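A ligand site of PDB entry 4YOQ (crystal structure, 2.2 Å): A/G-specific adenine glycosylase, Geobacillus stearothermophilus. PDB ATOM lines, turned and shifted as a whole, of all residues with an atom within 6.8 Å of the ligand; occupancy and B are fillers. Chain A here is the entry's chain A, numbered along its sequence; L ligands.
FE3 of the ligand is bound by SG of Cys 211 (2.4 Å).
SG of Cys 201 binds FE2 of the ligand (2.5 Å).
SG of Cys 208 binds FE1 of the ligand (2.5 Å).
An iron atom (FE4) of the ligand is bound by the side-chain sulfur of Cys 217 (2.5 Å).
The backbone NH of Cys 201 lies within hydrogen-bond range of the backbone carbonyl oxygen of Leu 196, 2.7 Å away.
The side-chain sulfur of Cys 208 sits close to the backbone carbonyl oxygen of Pro 206 (3.7 Å).
The side-chain sulfur of Cys 217 lies close to the backbone carbonyl oxygen of Arg 156, at 3.3 Å.
The side-chain sulfur of Cys 217 lies close to the backbone NH of Phe 220 (3.4 Å).
O of Arg 156 sits at hydrogen-bond distance from N of Ala 219.
O of Thr 202 sits at hydrogen-bond distance from NH1 of Arg 156 (2.8 Å).
O of Leu 157 is in hydrogen-bond range of N of Gln 218.
The backbone NH of Ser 207 sits at hydrogen-bond distance from the backbone carbonyl oxygen of Val 200 (3.0 Å).
Residues that only touch the ligand: Arg 156, Leu 157, Val 200, Gln 214 and Ala 225.
Hydrophobic or aromatic side chains that line the ligand: Leu 157, Val 200 and Ala 225.
Nine residues have an atom within 4 Å of the ligand: Arg 156, Leu 157, Val 200, Cys 201, Cys 208, Cys 211, Gln 214, Cys 217 and Ala 225.
The nearest printed residue that does not touch the ligand is Phe 220 (4.2 Å).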
ATOM      1  N   ARG A 152      -8.414 -21.464   7.713  1.00  0.00           N
ATOM      2  CA  ARG A 152      -7.991 -21.432   9.107  1.00  0.00           C
ATOM      3  C   ARG A 152      -8.761 -20.365   9.900  1.00  0.00           C
ATOM      4  O   ARG A 152      -9.150 -20.580  11.034  1.00  0.00           O
ATOM      5  CB  ARG A 152      -6.486 -21.201   9.226  1.00  0.00           C
ATOM      6  CG  ARG A 152      -5.953 -21.361  10.662  1.00  0.00           C
ATOM      7  CD  ARG A 152      -4.430 -21.372  10.710  1.00  0.00           C
ATOM      8  NE  ARG A 152      -3.882 -20.123  10.176  1.00  0.00           N
ATOM      9  CZ  ARG A 152      -3.305 -19.987   8.976  1.00  0.00           C
ATOM     10  NH1 ARG A 152      -3.174 -21.038   8.165  1.00  0.00           N
ATOM     11  NH2 ARG A 152      -2.859 -18.807   8.606  1.00  0.00           N
ATOM     12  N   VAL A 153      -8.966 -19.206   9.288  1.00  0.00           N
ATOM     13  CA  VAL A 153      -9.624 -18.120  10.005  1.00  0.00           C
ATOM     14  C   VAL A 153     -11.092 -18.487  10.210  1.00  0.00           C
ATOM     15  O   VAL A 153     -11.616 -18.414  11.313  1.00  0.00           O
ATOM     16  CB  VAL A 153      -9.482 -16.786   9.238  1.00  0.00           C
ATOM     17  CG1 VAL A 153     -10.286 -15.686   9.926  1.00  0.00           C
ATOM     18  CG2 VAL A 153      -8.029 -16.385   9.172  1.00  0.00           C
ATOM     19  N   ARG A 156     -11.774 -21.089  12.858  1.00  0.00           N
ATOM     20  CA  ARG A 156     -11.684 -20.625  14.223  1.00  0.00           C
ATOM     21  C   ARG A 156     -12.852 -19.691  14.519  1.00  0.00           C
ATOM     22  O   ARG A 156     -13.484 -19.777  15.566  1.00  0.00           O
ATOM     23  CB  ARG A 156     -10.339 -19.933  14.487  1.00  0.00           C
ATOM     24  CG  ARG A 156      -9.155 -20.895  14.658  1.00  0.00           C
ATOM     25  CD  ARG A 156      -7.812 -20.150  14.464  1.00  0.00           C
ATOM     26  NE  ARG A 156      -6.674 -21.064  14.544  1.00  0.00           N
ATOM     27  CZ  ARG A 156      -5.400 -20.724  14.369  1.00  0.00           C
ATOM     28  NH1 ARG A 156      -5.057 -19.470  14.107  1.00  0.00           N
ATOM     29  NH2 ARG A 156      -4.442 -21.655  14.461  1.00  0.00           N
ATOM     30  N   LEU A 157     -13.163 -18.811  13.567  1.00  0.00           N
ATOM     31  CA  LEU A 157     -14.211 -17.819  13.768  1.00  0.00           C
ATOM     32  C   LEU A 157     -15.561 -18.462  13.997  1.00  0.00           C
ATOM     33  O   LEU A 157     -16.356 -17.966  14.785  1.00  0.00           O
ATOM     34  CB  LEU A 157     -14.303 -16.867  12.581  1.00  0.00           C
ATOM     35  CG  LEU A 157     -13.368 -15.678  12.625  1.00  0.00           C
ATOM     36  CD1 LEU A 157     -13.484 -14.902  11.324  1.00  0.00           C
ATOM     37  CD2 LEU A 157     -13.686 -14.770  13.817  1.00  0.00           C
ATOM     38  N   LEU A 196      -5.219 -11.413   7.503  1.00  0.00           N
ATOM     39  CA  LEU A 196      -5.425 -11.796   8.901  1.00  0.00           C
ATOM     40  C   LEU A 196      -4.857 -13.186   9.198  1.00  0.00           C
ATOM     41  O   LEU A 196      -4.179 -13.386  10.190  1.00  0.00           O
ATOM     42  CB  LEU A 196      -6.897 -11.684   9.311  1.00  0.00           C
ATOM     43  CG  LEU A 196      -7.275 -11.877  10.781  1.00  0.00           C
ATOM     44  CD1 LEU A 196      -7.008 -10.619  11.639  1.00  0.00           C
ATOM     45  CD2 LEU A 196      -8.747 -12.301  10.945  1.00  0.00           C
ATOM     46  N   VAL A 200      -1.931 -12.420  11.791  1.00  0.00           N
ATOM     47  CA  VAL A 200      -2.460 -12.492  13.141  1.00  0.00           C
ATOM     48  C   VAL A 200      -2.942 -13.905  13.504  1.00  0.00           C
ATOM     49  O   VAL A 200      -2.528 -14.487  14.508  1.00  0.00           O
ATOM     50  CB  VAL A 200      -3.613 -11.469  13.298  1.00  0.00           C
ATOM     51  CG1 VAL A 200      -4.471 -11.806  14.508  1.00  0.00           C
ATOM     52  CG2 VAL A 200      -3.041 -10.047  13.373  1.00  0.00           C
ATOM     53  N   CYS A 201      -3.851 -14.434  12.692  1.00  0.00           N
ATOM     54  CA  CYS A 201      -4.495 -15.715  12.960  1.00  0.00           C
ATOM     55  C   CYS A 201      -3.726 -16.873  12.326  1.00  0.00           C
ATOM     56  O   CYS A 201      -4.173 -17.460  11.366  1.00  0.00           O
ATOM     57  CB  CYS A 201      -5.902 -15.712  12.394  1.00  0.00           C
ATOM     58  SG  CYS A 201      -6.822 -17.182  12.877  1.00  0.00           S
ATOM     59  N   THR A 202      -2.576 -17.200  12.903  1.00  0.00           N
ATOM     60  CA  THR A 202      -1.551 -17.981  12.213  1.00  0.00           C
ATOM     61  C   THR A 202      -1.624 -19.438  12.622  1.00  0.00           C
ATOM     62  O   THR A 202      -2.311 -19.772  13.604  1.00  0.00           O
ATOM     63  CB  THR A 202      -0.169 -17.413  12.625  1.00  0.00           C
ATOM     64  OG1 THR A 202      -0.080 -17.411  14.054  1.00  0.00           O
ATOM     65  CG2 THR A 202      -0.036 -15.987  12.132  1.00  0.00           C
ATOM     66  N   PRO A 206      -1.604 -18.200  17.581  1.00  0.00           N
ATOM     67  CA  PRO A 206      -2.275 -17.035  16.993  1.00  0.00           C
ATOM     68  C   PRO A 206      -2.410 -15.905  18.000  1.00  0.00           C
ATOM     69  O   PRO A 206      -2.664 -16.122  19.189  1.00  0.00           O
ATOM     70  CB  PRO A 206      -3.646 -17.572  16.613  1.00  0.00           C
ATOM     71  CG  PRO A 206      -3.881 -18.674  17.574  1.00  0.00           C
ATOM     72  CD  PRO A 206      -2.540 -19.328  17.747  1.00  0.00           C
ATOM     73  N   SER A 207      -2.289 -14.688  17.499  1.00  0.00           N
ATOM     74  CA  SER A 207      -2.269 -13.521  18.342  1.00  0.00           C
ATOM     75  C   SER A 207      -3.670 -12.970  18.566  1.00  0.00           C
ATOM     76  O   SER A 207      -3.969 -11.816  18.236  1.00  0.00           O
ATOM     77  CB  SER A 207      -1.352 -12.480  17.733  1.00  0.00           C
ATOM     78  OG  SER A 207      -0.083 -13.067  17.527  1.00  0.00           O
ATOM     79  N   CYS A 208      -4.523 -13.841  19.139  1.00  0.00           N
ATOM     80  CA  CYS A 208      -5.913 -13.556  19.473  1.00  0.00           C
ATOM     81  C   CYS A 208      -6.035 -12.275  20.342  1.00  0.00           C
ATOM     82  O   CYS A 208      -6.987 -11.491  20.210  1.00  0.00           O
ATOM     83  CB  CYS A 208      -6.527 -14.775  20.206  1.00  0.00           C
ATOM     84  SG  CYS A 208      -6.292 -16.480  19.406  1.00  0.00           S
ATOM     85  N   LEU A 209      -5.066 -12.035  21.215  1.00  0.00           N
ATOM     86  CA  LEU A 209      -5.112 -10.845  22.075  1.00  0.00           C
ATOM     87  C   LEU A 209      -5.035  -9.534  21.277  1.00  0.00           C
ATOM     88  O   LEU A 209      -5.686  -8.559  21.640  1.00  0.00           O
ATOM     89  CB  LEU A 209      -4.000 -10.901  23.125  1.00  0.00           C
ATOM     90  CG  LEU A 209      -4.165 -12.100  24.065  1.00  0.00           C
ATOM     91  CD1 LEU A 209      -3.094 -12.090  25.136  1.00  0.00           C
ATOM     92  CD2 LEU A 209      -5.558 -12.097  24.682  1.00  0.00           C
ATOM     93  N   LEU A 210      -4.262  -9.562  20.205  1.00  0.00           N
ATOM     94  CA  LEU A 210      -4.175  -8.459  19.252  1.00  0.00           C
ATOM     95  C   LEU A 210      -5.268  -8.458  18.152  1.00  0.00           C
ATOM     96  O   LEU A 210      -5.445  -7.441  17.482  1.00  0.00           O
ATOM     97  CB  LEU A 210      -2.833  -8.505  18.534  1.00  0.00           C
ATOM     98  CG  LEU A 210      -1.567  -8.388  19.382  1.00  0.00           C
ATOM     99  CD1 LEU A 210      -0.344  -8.690  18.521  1.00  0.00           C
ATOM    100  CD2 LEU A 210      -1.477  -7.002  20.005  1.00  0.00           C
ATOM    101  N   CYS A 211      -5.987  -9.566  17.960  1.00  0.00           N
ATOM    102  CA  CYS A 211      -6.849  -9.667  16.788  1.00  0.00           C
ATOM    103  C   CYS A 211      -8.053  -8.733  16.797  1.00  0.00           C
ATOM    104  O   CYS A 211      -8.760  -8.649  17.806  1.00  0.00           O
ATOM    105  CB  CYS A 211      -7.333 -11.110  16.549  1.00  0.00           C
ATOM    106  SG  CYS A 211      -8.485 -11.211  15.149  1.00  0.00           S
ATOM    107  N   PRO A 212      -8.318  -8.070  15.655  1.00  0.00           N
ATOM    108  CA  PRO A 212      -9.394  -7.087  15.515  1.00  0.00           C
ATOM    109  C   PRO A 212     -10.790  -7.674  15.286  1.00  0.00           C
ATOM    110  O   PRO A 212     -11.739  -6.901  15.141  1.00  0.00           O
ATOM    111  CB  PRO A 212      -8.995  -6.334  14.259  1.00  0.00           C
ATOM    112  CG  PRO A 212      -8.357  -7.441  13.428  1.00  0.00           C
ATOM    113  CD  PRO A 212      -7.528  -8.184  14.417  1.00  0.00           C
ATOM    114  N   VAL A 213     -10.917  -8.997  15.202  1.00  0.00           N
ATOM    115  CA  VAL A 213     -12.234  -9.596  15.076  1.00  0.00           C
ATOM    116  C   VAL A 213     -12.420 -10.627  16.168  1.00  0.00           C
ATOM    117  O   VAL A 213     -13.288 -11.509  16.071  1.00  0.00           O
ATOM    118  CB  VAL A 213     -12.468 -10.224  13.662  1.00  0.00           C
ATOM    119  CG1 VAL A 213     -12.467  -9.135  12.586  1.00  0.00           C
ATOM    120  CG2 VAL A 213     -11.429 -11.286  13.362  1.00  0.00           C
ATOM    121  N   GLN A 214     -11.606 -10.490  17.214  1.00  0.00           N
ATOM    122  CA  GLN A 214     -11.638 -11.350  18.389  1.00  0.00           C
ATOM    123  C   GLN A 214     -13.019 -11.439  19.039  1.00  0.00           C
ATOM    124  O   GLN A 214     -13.400 -12.503  19.555  1.00  0.00           O
ATOM    125  CB  GLN A 214     -10.663 -10.835  19.440  1.00  0.00           C
ATOM    126  CG  GLN A 214     -10.524 -11.749  20.643  1.00  0.00           C
ATOM    127  CD  GLN A 214     -10.259 -10.979  21.915  1.00  0.00           C
ATOM    128  OE1 GLN A 214     -11.140 -10.278  22.412  1.00  0.00           O
ATOM    129  NE2 GLN A 214      -9.052 -11.101  22.437  1.00  0.00           N
ATOM    130  N   ALA A 215     -13.751 -10.336  19.042  1.00  0.00           N
ATOM    131  CA  ALA A 215     -15.058 -10.311  19.690  1.00  0.00           C
ATOM    132  C   ALA A 215     -15.973 -11.316  19.021  1.00  0.00           C
ATOM    133  O   ALA A 215     -16.756 -11.981  19.687  1.00  0.00           O
ATOM    134  CB  ALA A 215     -15.656  -8.908  19.650  1.00  0.00           C
ATOM    135  N   TYR A 216     -15.820 -11.457  17.708  1.00  0.00           N
ATOM    136  CA  TYR A 216     -16.665 -12.334  16.905  1.00  0.00           C
ATOM    137  C   TYR A 216     -16.180 -13.768  16.847  1.00  0.00           C
ATOM    138  O   TYR A 216     -16.711 -14.567  16.077  1.00  0.00           O
ATOM    139  CB  TYR A 216     -16.782 -11.817  15.473  1.00  0.00           C
ATOM    140  CG  TYR A 216     -16.981 -10.324  15.324  1.00  0.00           C
ATOM    141  CD1 TYR A 216     -15.910  -9.484  15.051  1.00  0.00           C
ATOM    142  CD2 TYR A 216     -18.246  -9.740  15.424  1.00  0.00           C
ATOM    143  CE1 TYR A 216     -16.076  -8.121  14.901  1.00  0.00           C
ATOM    144  CE2 TYR A 216     -18.420  -8.371  15.275  1.00  0.00           C
ATOM    145  CZ  TYR A 216     -17.334  -7.568  15.011  1.00  0.00           C
ATOM    146  OH  TYR A 216     -17.477  -6.206  14.861  1.00  0.00           O
ATOM    147  N   CYS A 217     -15.185 -14.132  17.652  1.00  0.00           N
ATOM    148  CA  CYS A 217     -14.577 -15.439  17.439  1.00  0.00           C
ATOM    149  C   CYS A 217     -14.887 -16.524  18.447  1.00  0.00           C
ATOM    150  O   CYS A 217     -14.397 -16.500  19.575  1.00  0.00           O
ATOM    151  CB  CYS A 217     -13.066 -15.352  17.298  1.00  0.00           C
ATOM    152  SG  CYS A 217     -12.408 -17.031  17.150  1.00  0.00           S
ATOM    153  N   GLN A 218     -15.627 -17.528  17.994  1.00  0.00           N
ATOM    154  CA  GLN A 218     -16.064 -18.628  18.845  1.00  0.00           C
ATOM    155  C   GLN A 218     -14.904 -19.481  19.338  1.00  0.00           C
ATOM    156  O   GLN A 218     -14.927 -19.949  20.457  1.00  0.00           O
ATOM    157  CB  GLN A 218     -17.075 -19.514  18.110  1.00  0.00           C
ATOM    158  CG  GLN A 218     -18.259 -18.777  17.503  1.00  0.00           C
ATOM    159  CD  GLN A 218     -19.229 -19.734  16.829  1.00  0.00           C
ATOM    160  OE1 GLN A 218     -19.417 -20.865  17.274  1.00  0.00           O
ATOM    161  NE2 GLN A 218     -19.843 -19.279  15.735  1.00  0.00           N
ATOM    162  N   ALA A 219     -13.882 -19.698  18.513  1.00  0.00           N
ATOM    163  CA  ALA A 219     -12.776 -20.534  18.979  1.00  0.00           C
ATOM    164  C   ALA A 219     -12.045 -19.926  20.184  1.00  0.00           C
ATOM    165  O   ALA A 219     -11.666 -20.631  21.113  1.00  0.00           O
ATOM    166  CB  ALA A 219     -11.804 -20.841  17.868  1.00  0.00           C
ATOM    167  N   PHE A 220     -11.869 -18.604  20.153  1.00  0.00           N
ATOM    168  CA  PHE A 220     -11.241 -17.903  21.272  1.00  0.00           C
ATOM    169  C   PHE A 220     -12.123 -17.983  22.527  1.00  0.00           C
ATOM    170  O   PHE A 220     -11.655 -18.319  23.606  1.00  0.00           O
ATOM    171  CB  PHE A 220     -10.962 -16.441  20.911  1.00  0.00           C
ATOM    172  CG  PHE A 220     -10.359 -15.640  22.032  1.00  0.00           C
ATOM    173  CD1 PHE A 220      -9.031 -15.832  22.405  1.00  0.00           C
ATOM    174  CD2 PHE A 220     -11.096 -14.685  22.703  1.00  0.00           C
ATOM    175  CE1 PHE A 220      -8.463 -15.086  23.433  1.00  0.00           C
ATOM    176  CE2 PHE A 220     -10.540 -13.918  23.727  1.00  0.00           C
ATOM    177  CZ  PHE A 220      -9.221 -14.124  24.085  1.00  0.00           C
ATOM    178  N   ALA A 225      -8.698 -21.877  19.859  1.00  0.00           N
ATOM    179  CA  ALA A 225      -8.064 -21.319  18.646  1.00  0.00           C
ATOM    180  C   ALA A 225      -6.910 -22.172  18.146  1.00  0.00           C
ATOM    181  O   ALA A 225      -6.806 -22.459  16.950  1.00  0.00           O
ATOM    182  CB  ALA A 225      -7.599 -19.884  18.871  1.00  0.00           C
ATOM    183  N   GLU A 226      -6.066 -22.600  19.084  1.00  0.00           N
ATOM    184  CA  GLU A 226      -4.880 -23.389  18.764  1.00  0.00           C
ATOM    185  C   GLU A 226      -5.146 -24.781  18.145  1.00  0.00           C
ATOM    186  O   GLU A 226      -4.305 -25.325  17.448  1.00  0.00           O
ATOM    187  CB  GLU A 226      -4.005 -23.520  20.016  1.00  0.00           C
ATOM    188  CG  GLU A 226      -2.601 -24.018  19.778  1.00  0.00           C
ATOM    189  CD  GLU A 226      -1.531 -22.965  20.044  1.00  0.00           C
ATOM    190  OE1 GLU A 226      -0.613 -22.817  19.193  1.00  0.00           O
ATOM    191  OE2 GLU A 226      -1.599 -22.301  21.115  1.00  0.00           O
HETATM  192 FE1  LIG L   1      -7.707 -15.476  17.649  1.00  0.00          FE
HETATM  193 FE2  LIG L   1      -8.057 -16.254  14.786  1.00  0.00          FE
HETATM  194 FE3  LIG L   1      -8.678 -13.570  15.723  1.00  0.00          FE
HETATM  195 FE4  LIG L   1     -10.316 -15.960  16.374  1.00  0.00          FE
HETATM  196  S1  LIG L   1      -9.799 -15.029  14.483  1.00  0.00           S
HETATM  197  S2  LIG L   1      -9.483 -14.308  17.600  1.00  0.00           S
HETATM  198  S3  LIG L   1      -8.584 -17.219  16.655  1.00  0.00           S
HETATM  199  S4  LIG L   1      -6.859 -14.695  15.819  1.00  0.00           S
